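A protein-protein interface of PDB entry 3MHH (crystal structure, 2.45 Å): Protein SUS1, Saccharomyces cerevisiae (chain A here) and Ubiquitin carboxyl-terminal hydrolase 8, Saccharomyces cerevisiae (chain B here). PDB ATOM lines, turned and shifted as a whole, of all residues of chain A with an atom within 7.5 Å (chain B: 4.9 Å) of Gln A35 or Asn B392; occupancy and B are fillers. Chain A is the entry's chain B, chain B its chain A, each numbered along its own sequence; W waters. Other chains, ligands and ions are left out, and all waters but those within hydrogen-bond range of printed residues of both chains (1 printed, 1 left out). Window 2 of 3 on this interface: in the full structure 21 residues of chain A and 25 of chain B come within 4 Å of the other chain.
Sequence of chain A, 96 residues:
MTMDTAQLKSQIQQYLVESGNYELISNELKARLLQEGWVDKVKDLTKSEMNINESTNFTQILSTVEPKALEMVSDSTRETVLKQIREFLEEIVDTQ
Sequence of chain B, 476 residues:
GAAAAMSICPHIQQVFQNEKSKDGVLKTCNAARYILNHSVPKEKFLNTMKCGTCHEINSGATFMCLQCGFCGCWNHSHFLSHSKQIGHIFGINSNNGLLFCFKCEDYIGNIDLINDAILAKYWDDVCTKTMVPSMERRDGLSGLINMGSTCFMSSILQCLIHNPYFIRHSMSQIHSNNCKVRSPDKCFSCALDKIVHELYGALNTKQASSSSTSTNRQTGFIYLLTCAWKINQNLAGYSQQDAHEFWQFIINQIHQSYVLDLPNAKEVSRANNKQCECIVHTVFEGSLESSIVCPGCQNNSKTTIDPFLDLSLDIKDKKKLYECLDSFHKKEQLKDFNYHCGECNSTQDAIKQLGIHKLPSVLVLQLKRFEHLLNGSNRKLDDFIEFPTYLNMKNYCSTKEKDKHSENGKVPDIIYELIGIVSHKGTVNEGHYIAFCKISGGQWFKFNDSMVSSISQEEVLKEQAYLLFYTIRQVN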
ATOM      1  N   GLU A  28      17.711 -14.715 -10.737  1.00  0.00           N
ATOM      2  CA  GLU A  28      17.274 -16.058 -11.130  1.00  0.00           C
ATOM      3  C   GLU A  28      18.460 -16.784 -11.724  1.00  0.00           C
ATOM      4  O   GLU A  28      18.720 -17.954 -11.418  1.00  0.00           O
ATOM      5  CB  GLU A  28      16.141 -15.961 -12.156  1.00  0.00           C
ATOM      6  CG  GLU A  28      15.737 -17.274 -12.801  1.00  0.00           C
ATOM      7  CD  GLU A  28      14.810 -18.109 -11.941  1.00  0.00           C
ATOM      8  OE1 GLU A  28      14.319 -19.151 -12.452  1.00  0.00           O
ATOM      9  OE2 GLU A  28      14.582 -17.740 -10.764  1.00  0.00           O
ATOM     10  N   LEU A  29      19.210 -16.059 -12.541  1.00  0.00           N
ATOM     11  CA  LEU A  29      20.380 -16.614 -13.194  1.00  0.00           C
ATOM     12  C   LEU A  29      21.414 -16.984 -12.155  1.00  0.00           C
ATOM     13  O   LEU A  29      22.004 -18.056 -12.207  1.00  0.00           O
ATOM     14  CB  LEU A  29      20.967 -15.605 -14.179  1.00  0.00           C
ATOM     15  CG  LEU A  29      22.297 -16.009 -14.806  1.00  0.00           C
ATOM     16  CD1 LEU A  29      22.157 -17.279 -15.613  1.00  0.00           C
ATOM     17  CD2 LEU A  29      22.791 -14.888 -15.663  1.00  0.00           C
ATOM     18  N   LYS A  30      21.657 -16.073 -11.223  1.00  0.00           N
ATOM     19  CA  LYS A  30      22.580 -16.341 -10.136  1.00  0.00           C
ATOM     20  C   LYS A  30      22.130 -17.560  -9.320  1.00  0.00           C
ATOM     21  O   LYS A  30      22.894 -18.508  -9.163  1.00  0.00           O
ATOM     22  CB  LYS A  30      22.741 -15.103  -9.251  1.00  0.00           C
ATOM     23  CG  LYS A  30      23.516 -13.992  -9.940  1.00  0.00           C
ATOM     24  CD  LYS A  30      23.786 -12.789  -9.012  1.00  0.00           C
ATOM     25  CE  LYS A  30      24.375 -11.605  -9.780  1.00  0.00           C
ATOM     26  NZ  LYS A  30      24.619 -10.427  -8.900  1.00  0.00           N
ATOM     27  N   ALA A  31      20.888 -17.564  -8.843  1.00  0.00           N
ATOM     28  CA  ALA A  31      20.368 -18.728  -8.105  1.00  0.00           C
ATOM     29  C   ALA A  31      20.672 -20.043  -8.825  1.00  0.00           C
ATOM     30  O   ALA A  31      21.148 -20.997  -8.212  1.00  0.00           O
ATOM     31  CB  ALA A  31      18.863 -18.609  -7.869  1.00  0.00           C
ATOM     32  N   ARG A  32      20.363 -20.103 -10.118  1.00  0.00           N
ATOM     33  CA  ARG A  32      20.569 -21.323 -10.878  1.00  0.00           C
ATOM     34  C   ARG A  32      22.047 -21.682 -11.008  1.00  0.00           C
ATOM     35  O   ARG A  32      22.433 -22.825 -10.788  1.00  0.00           O
ATOM     36  CB  ARG A  32      19.915 -21.221 -12.255  1.00  0.00           C
ATOM     37  CG  ARG A  32      18.380 -21.285 -12.211  1.00  0.00           C
ATOM     38  CD  ARG A  32      17.748 -21.032 -13.591  1.00  0.00           C
ATOM     39  NE  ARG A  32      16.284 -21.080 -13.531  1.00  0.00           N
ATOM     40  CZ  ARG A  32      15.564 -22.200 -13.618  1.00  0.00           C
ATOM     41  NH1 ARG A  32      16.156 -23.375 -13.801  1.00  0.00           N
ATOM     42  NH2 ARG A  32      14.243 -22.148 -13.520  1.00  0.00           N
ATOM     43  N   LEU A  33      22.881 -20.711 -11.350  1.00  0.00           N
ATOM     44  CA  LEU A  33      24.284 -21.001 -11.591  1.00  0.00           C
ATOM     45  C   LEU A  33      24.968 -21.451 -10.295  1.00  0.00           C
ATOM     46  O   LEU A  33      25.820 -22.345 -10.284  1.00  0.00           O
ATOM     47  CB  LEU A  33      24.975 -19.771 -12.170  1.00  0.00           C
ATOM     48  CG  LEU A  33      24.540 -19.388 -13.583  1.00  0.00           C
ATOM     49  CD1 LEU A  33      25.064 -18.018 -13.955  1.00  0.00           C
ATOM     50  CD2 LEU A  33      25.006 -20.412 -14.582  1.00  0.00           C
ATOM     51  N   LEU A  34      24.583 -20.820  -9.198  1.00  0.00           N
ATOM     52  CA  LEU A  34      25.072 -21.208  -7.891  1.00  0.00           C
ATOM     53  C   LEU A  34      24.649 -22.641  -7.594  1.00  0.00           C
ATOM     54  O   LEU A  34      25.476 -23.470  -7.232  1.00  0.00           O
ATOM     55  CB  LEU A  34      24.522 -20.251  -6.835  1.00  0.00           C
ATOM     56  CG  LEU A  34      24.919 -20.500  -5.387  1.00  0.00           C
ATOM     57  CD1 LEU A  34      26.418 -20.240  -5.181  1.00  0.00           C
ATOM     58  CD2 LEU A  34      24.058 -19.618  -4.474  1.00  0.00           C
ATOM     59  N   GLN A  35      23.365 -22.940  -7.770  1.00  0.00           N
ATOM     60  CA  GLN A  35      22.819 -24.250  -7.389  1.00  0.00           C
ATOM     61  C   GLN A  35      23.344 -25.399  -8.252  1.00  0.00           C
ATOM     62  O   GLN A  35      23.557 -26.504  -7.758  1.00  0.00           O
ATOM     63  CB  GLN A  35      21.285 -24.238  -7.420  1.00  0.00           C
ATOM     64  CG  GLN A  35      20.636 -23.725  -6.116  1.00  0.00           C
ATOM     65  CD  GLN A  35      19.122 -23.608  -6.215  1.00  0.00           C
ATOM     66  OE1 GLN A  35      18.392 -24.314  -5.526  1.00  0.00           O
ATOM     67  NE2 GLN A  35      18.644 -22.717  -7.086  1.00  0.00           N
ATOM     68  N   GLU A  36      23.563 -25.148  -9.533  1.00  0.00           N
ATOM     69  CA  GLU A  36      24.044 -26.204 -10.414  1.00  0.00           C
ATOM     70  C   GLU A  36      25.554 -26.414 -10.322  1.00  0.00           C
ATOM     71  O   GLU A  36      26.100 -27.243 -11.047  1.00  0.00           O
ATOM     72  CB  GLU A  36      23.635 -25.934 -11.861  1.00  0.00           C
ATOM     73  CG  GLU A  36      24.566 -24.989 -12.621  1.00  0.00           C
ATOM     74  CD  GLU A  36      23.994 -24.613 -13.976  1.00  0.00           C
ATOM     75  OE1 GLU A  36      22.752 -24.571 -14.076  1.00  0.00           O
ATOM     76  OE2 GLU A  36      24.780 -24.373 -14.924  1.00  0.00           O
ATOM     77  N   GLY A  37      26.220 -25.658  -9.446  1.00  0.00           N
ATOM     78  CA  GLY A  37      27.657 -25.833  -9.187  1.00  0.00           C
ATOM     79  C   GLY A  37      28.605 -24.985 -10.023  1.00  0.00           C
ATOM     80  O   GLY A  37      29.833 -25.090  -9.887  1.00  0.00           O
ATOM     81  N   TRP A  38      28.046 -24.131 -10.877  1.00  0.00           N
ATOM     82  CA  TRP A  38      28.834 -23.372 -11.846  1.00  0.00           C
ATOM     83  C   TRP A  38      29.734 -22.306 -11.211  1.00  0.00           C
ATOM     84  O   TRP A  38      30.867 -22.110 -11.642  1.00  0.00           O
ATOM     85  CB  TRP A  38      27.898 -22.734 -12.854  1.00  0.00           C
ATOM     86  CG  TRP A  38      28.545 -21.902 -13.891  1.00  0.00           C
ATOM     87  CD1 TRP A  38      28.883 -22.285 -15.141  1.00  0.00           C
ATOM     88  CD2 TRP A  38      28.855 -20.506 -13.800  1.00  0.00           C
ATOM     89  NE1 TRP A  38      29.416 -21.226 -15.838  1.00  0.00           N
ATOM     90  CE2 TRP A  38      29.414 -20.123 -15.031  1.00  0.00           C
ATOM     91  CE3 TRP A  38      28.736 -19.551 -12.788  1.00  0.00           C
ATOM     92  CZ2 TRP A  38      29.841 -18.828 -15.283  1.00  0.00           C
ATOM     93  CZ3 TRP A  38      29.148 -18.265 -13.045  1.00  0.00           C
ATOM     94  CH2 TRP A  38      29.696 -17.913 -14.278  1.00  0.00           C
ATOM     95  N   VAL A  39      29.240 -21.620 -10.189  1.00  0.00           N
ATOM     96  CA  VAL A  39      30.032 -20.586  -9.539  1.00  0.00           C
ATOM     97  C   VAL A  39      31.339 -21.172  -9.003  1.00  0.00           C
ATOM     98  O   VAL A  39      32.412 -20.629  -9.242  1.00  0.00           O
ATOM     99  CB  VAL A  39      29.227 -19.855  -8.444  1.00  0.00           C
ATOM    100  CG1 VAL A  39      30.143 -19.056  -7.530  1.00  0.00           C
ATOM    101  CG2 VAL A  39      28.179 -18.934  -9.092  1.00  0.00           C
ATOM    102  N   ASP A  40      31.250 -22.310  -8.333  1.00  0.00           N
ATOM    103  CA  ASP A  40      32.418 -22.948  -7.730  1.00  0.00           C
ATOM    104  C   ASP A  40      33.294 -23.638  -8.774  1.00  0.00           C
ATOM    105  O   ASP A  40      34.504 -23.771  -8.590  1.00  0.00           O
ATOM    106  CB  ASP A  40      31.957 -23.911  -6.637  1.00  0.00           C
ATOM    107  CG  ASP A  40      31.119 -23.207  -5.603  1.00  0.00           C
ATOM    108  OD1 ASP A  40      31.437 -22.038  -5.311  1.00  0.00           O
ATOM    109  OD2 ASP A  40      30.123 -23.770  -5.122  1.00  0.00           O
ATOM    110  N   TYR B 322      16.233 -33.626   1.040  1.00  0.00           N
ATOM    111  CA  TYR B 322      14.988 -32.985   0.669  1.00  0.00           C
ATOM    112  C   TYR B 322      13.812 -33.843   1.103  1.00  0.00           C
ATOM    113  O   TYR B 322      12.846 -33.329   1.667  1.00  0.00           O
ATOM    114  CB  TYR B 322      14.920 -32.666  -0.827  1.00  0.00           C
ATOM    115  CG  TYR B 322      15.625 -31.378  -1.190  1.00  0.00           C
ATOM    116  CD1 TYR B 322      15.289 -30.176  -0.563  1.00  0.00           C
ATOM    117  CD2 TYR B 322      16.632 -31.358  -2.149  1.00  0.00           C
ATOM    118  CE1 TYR B 322      15.934 -28.992  -0.897  1.00  0.00           C
ATOM    119  CE2 TYR B 322      17.279 -30.189  -2.476  1.00  0.00           C
ATOM    120  CZ  TYR B 322      16.928 -29.011  -1.851  1.00  0.00           C
ATOM    121  OH  TYR B 322      17.592 -27.853  -2.179  1.00  0.00           O
ATOM    122  N   TYR B 390      24.347 -26.974  -1.894  1.00  0.00           N
ATOM    123  CA  TYR B 390      23.487 -25.807  -1.714  1.00  0.00           C
ATOM    124  C   TYR B 390      22.058 -26.264  -1.520  1.00  0.00           C
ATOM    125  O   TYR B 390      21.517 -27.025  -2.333  1.00  0.00           O
ATOM    126  CB  TYR B 390      23.575 -24.877  -2.924  1.00  0.00           C
ATOM    127  CG  TYR B 390      24.931 -24.252  -3.073  1.00  0.00           C
ATOM    128  CD1 TYR B 390      25.256 -23.086  -2.401  1.00  0.00           C
ATOM    129  CD2 TYR B 390      25.896 -24.830  -3.876  1.00  0.00           C
ATOM    130  CE1 TYR B 390      26.506 -22.513  -2.520  1.00  0.00           C
ATOM    131  CE2 TYR B 390      27.151 -24.259  -4.007  1.00  0.00           C
ATOM    132  CZ  TYR B 390      27.449 -23.106  -3.312  1.00  0.00           C
ATOM    133  OH  TYR B 390      28.695 -22.545  -3.425  1.00  0.00           O
ATOM    134  N   LEU B 391      21.449 -25.747  -0.463  1.00  0.00           N
ATOM    135  CA  LEU B 391      20.151 -26.186   0.002  1.00  0.00           C
ATOM    136  C   LEU B 391      19.175 -25.051  -0.211  1.00  0.00           C
ATOM    137  O   LEU B 391      19.410 -23.933   0.273  1.00  0.00           O
ATOM    138  CB  LEU B 391      20.238 -26.454   1.504  1.00  0.00           C
ATOM    139  CG  LEU B 391      19.288 -27.422   2.194  1.00  0.00           C
ATOM    140  CD1 LEU B 391      19.218 -27.074   3.682  1.00  0.00           C
ATOM    141  CD2 LEU B 391      17.936 -27.403   1.546  1.00  0.00           C
ATOM    142  N   ASN B 392      18.079 -25.341  -0.915  1.00  0.00           N
ATOM    143  CA  ASN B 392      17.027 -24.359  -1.137  1.00  0.00           C
ATOM    144  C   ASN B 392      15.890 -24.610  -0.151  1.00  0.00           C
ATOM    145  O   ASN B 392      15.246 -25.653  -0.184  1.00  0.00           O
ATOM    146  CB  ASN B 392      16.531 -24.416  -2.592  1.00  0.00           C
ATOM    147  CG  ASN B 392      15.808 -23.141  -3.024  1.00  0.00           C
ATOM    148  OD1 ASN B 392      15.230 -22.439  -2.201  1.00  0.00           O
ATOM    149  ND2 ASN B 392      15.835 -22.845  -4.326  1.00  0.00           N
ATOM    150  N   MET B 393      15.646 -23.651   0.735  1.00  0.00           N
ATOM    151  CA  MET B 393      14.671 -23.851   1.793  1.00  0.00           C
ATOM    152  C   MET B 393      13.270 -23.351   1.447  1.00  0.00           C
ATOM    153  O   MET B 393      12.369 -23.419   2.284  1.00  0.00           O
ATOM    154  CB  MET B 393      15.157 -23.184   3.084  1.00  0.00           C
ATOM    155  CG  MET B 393      16.322 -23.916   3.775  1.00  0.00           C
ATOM    156  SD  MET B 393      15.902 -25.615   4.148  1.00  0.00           S
ATOM    157  CE  MET B 393      14.598 -25.349   5.321  1.00  0.00           C
ATOM    158  N   LYS B 394      13.056 -22.920   0.207  1.00  0.00           N
ATOM    159  CA  LYS B 394      11.828 -22.220  -0.130  1.00  0.00           C
ATOM    160  C   LYS B 394      10.575 -23.061   0.039  1.00  0.00           C
ATOM    161  O   LYS B 394       9.532 -22.549   0.444  1.00  0.00           O
ATOM    162  CB  LYS B 394      11.897 -21.628  -1.542  1.00  0.00           C
ATOM    163  CG  LYS B 394      11.726 -22.610  -2.685  1.00  0.00           C
ATOM    164  CD  LYS B 394      11.936 -21.915  -4.025  1.00  0.00           C
ATOM    165  CE  LYS B 394      11.496 -22.780  -5.210  1.00  0.00           C
ATOM    166  NZ  LYS B 394      12.172 -22.338  -6.475  1.00  0.00           N
ATOM    167  N   ASN B 395      10.676 -24.353  -0.259  1.00  0.00           N
ATOM    168  CA  ASN B 395       9.522 -25.252  -0.157  1.00  0.00           C
ATOM    169  C   ASN B 395       9.074 -25.532   1.285  1.00  0.00           C
ATOM    170  O   ASN B 395       8.059 -26.172   1.502  1.00  0.00           O
ATOM    171  CB  ASN B 395       9.830 -26.587  -0.854  1.00  0.00           C
ATOM    172  CG  ASN B 395       9.732 -26.501  -2.375  1.00  0.00           C
ATOM    173  OD1 ASN B 395       9.123 -25.589  -2.921  1.00  0.00           O
ATOM    174  ND2 ASN B 395      10.323 -27.474  -3.062  1.00  0.00           N
ATOM    175  N   TYR B 396       9.815 -25.064   2.277  1.00  0.00           N
ATOM    176  CA  TYR B 396       9.516 -25.465   3.655  1.00  0.00           C
ATOM    177  C   TYR B 396       9.099 -24.296   4.534  1.00  0.00           C
ATOM    178  O   TYR B 396       8.855 -24.458   5.729  1.00  0.00           O
ATOM    179  CB  TYR B 396      10.720 -26.217   4.247  1.00  0.00           C
ATOM    180  CG  TYR B 396      11.158 -27.313   3.326  1.00  0.00           C
ATOM    181  CD1 TYR B 396      10.405 -28.475   3.198  1.00  0.00           C
ATOM    182  CD2 TYR B 396      12.255 -27.146   2.492  1.00  0.00           C
ATOM    183  CE1 TYR B 396      10.756 -29.463   2.298  1.00  0.00           C
ATOM    184  CE2 TYR B 396      12.613 -28.120   1.588  1.00  0.00           C
ATOM    185  CZ  TYR B 396      11.871 -29.287   1.501  1.00  0.00           C
ATOM    186  OH  TYR B 396      12.246 -30.265   0.604  1.00  0.00           O
ATOM    187  N   PRO B 412      10.293 -17.104  -2.459  1.00  0.00           N
ATOM    188  CA  PRO B 412      11.437 -17.017  -3.356  1.00  0.00           C
ATOM    189  C   PRO B 412      12.520 -18.048  -3.025  1.00  0.00           C
ATOM    190  O   PRO B 412      12.493 -18.665  -1.950  1.00  0.00           O
ATOM    191  CB  PRO B 412      11.954 -15.595  -3.112  1.00  0.00           C
ATOM    192  CG  PRO B 412      11.569 -15.299  -1.709  1.00  0.00           C
ATOM    193  CD  PRO B 412      10.245 -15.977  -1.510  1.00  0.00           C
ATOM    194  N   ASP B 413      13.461 -18.245  -3.944  1.00  0.00           N
ATOM    195  CA  ASP B 413      14.597 -19.088  -3.643  1.00  0.00           C
ATOM    196  C   ASP B 413      15.294 -18.507  -2.425  1.00  0.00           C
ATOM    197  O   ASP B 413      15.593 -17.313  -2.390  1.00  0.00           O
ATOM    198  CB  ASP B 413      15.576 -19.140  -4.809  1.00  0.00           C
ATOM    199  CG  ASP B 413      14.960 -19.710  -6.059  1.00  0.00           C
ATOM    200  OD1 ASP B 413      14.250 -20.749  -5.975  1.00  0.00           O
ATOM    201  OD2 ASP B 413      15.199 -19.103  -7.129  1.00  0.00           O
ATOM    202  N   ILE B 414      15.496 -19.351  -1.418  1.00  0.00           N
ATOM    203  CA  ILE B 414      16.305 -19.034  -0.249  1.00  0.00           C
ATOM    204  C   ILE B 414      17.387 -20.107  -0.116  1.00  0.00           C
ATOM    205  O   ILE B 414      17.123 -21.231   0.320  1.00  0.00           O
ATOM    206  CB  ILE B 414      15.459 -19.020   1.016  1.00  0.00           C
ATOM    207  CG1 ILE B 414      14.374 -17.960   0.895  1.00  0.00           C
ATOM    208  CG2 ILE B 414      16.335 -18.718   2.226  1.00  0.00           C
ATOM    209  CD1 ILE B 414      13.382 -17.959   2.050  1.00  0.00           C
ATOM    210  N   ILE B 415      18.607 -19.751  -0.498  1.00  0.00           N
ATOM    211  CA  ILE B 415      19.650 -20.730  -0.748  1.00  0.00           C
ATOM    212  C   ILE B 415      20.785 -20.630   0.255  1.00  0.00           C
ATOM    213  O   ILE B 415      21.374 -19.562   0.461  1.00  0.00           O
ATOM    214  CB  ILE B 415      20.212 -20.578  -2.178  1.00  0.00           C
ATOM    215  CG1 ILE B 415      19.083 -20.773  -3.210  1.00  0.00           C
ATOM    216  CG2 ILE B 415      21.306 -21.588  -2.416  1.00  0.00           C
ATOM    217  CD1 ILE B 415      19.415 -20.316  -4.606  1.00  0.00           C
HETATM  218  O   HOH W   1      15.416 -23.100  -7.905  1.00  0.00           O
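The side-chain hydroxyl of Tyr B390 lies within hydrogen-bond range of the side-chain carboxylate of Asp A40 (2.5 Å). The side-chain amide oxygen of Gln A35 lies within hydrogen-bond range of the side-chain amide nitrogen of Asn B392, at 3.2 Å.
The backbone NH of Asn B392 sits at hydrogen-bond distance from the side-chain hydroxyl of Tyr B322. OD1 of Asn B392 is in hydrogen-bond range of N of Lys B394, at 3.3 Å. N of Ile B414 sits at hydrogen-bond distance from OD1 of Asn B392 (3.2 Å). NZ of Lys B394 lies within salt-bridge range of OD1 of Asp B413 (2.7 Å). The side-chain carboxylate (OE1) of Glu A28 lies within salt-bridge range of the guanidinium group (NE) of Arg A32, 3.0 Å away. The backbone carbonyl oxygen of Ala A31 lies within hydrogen-bond range of the side-chain amide nitrogen of Gln A35, 3.2 Å away.
Glu A28 touches Asp B413. OD2 of Asp B413 touches CB of Ala A31 (3.8 Å). CD1 of Ile B415 touches CB of Ala A31 (3.7 Å). Tyr B390 touches Leu A34. CG2 of Ile B415 touches CD2 of Leu A34, 3.96 Å away. Ile B415 touches Gln A35.
Of the printed residues of chain B, Glu A28 touches Asp B413 (3.9 Å). Printed residues of chain B within 4 Å of Ala A31: Asp B413 (3.8 Å) and Ile B415 (3.7 Å). Of chain B, only Asn B392 and Ile B415 come within 4 Å of Gln A35. Printed residues of chain B within 4 Å of Asp A40: Tyr B390. Of the printed residues of chain A, Tyr B390 touches Leu A34 and Asp A40. Asn B392 touches just one residue of chain A: Gln A35. Printed residues of chain A within 4 Å of Asp B413: Glu A28 (3.9 Å) and Ala A31 (3.8 Å). The nearest printed residue of chain B that does not touch Leu A34 is Leu B391 (7.8 Å).
Of the 12 printed residues of chain B, 4 touch a printed residue of chain A. Hydrophobic or aromatic side chains of chain B that line the printed part of chain A: Tyr B390 and Ile B415. Hydrophobic or aromatic side chains of chain A that line the printed part of chain B: Ala A31 and Leu A34. Among the printed residues, 8 pairs touch across the chains.
Water W1 lies within hydrogen-bond range of OD1 of Asp B413 (3.3 Å) and NE2 of Gln A35 (3.4 Å).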
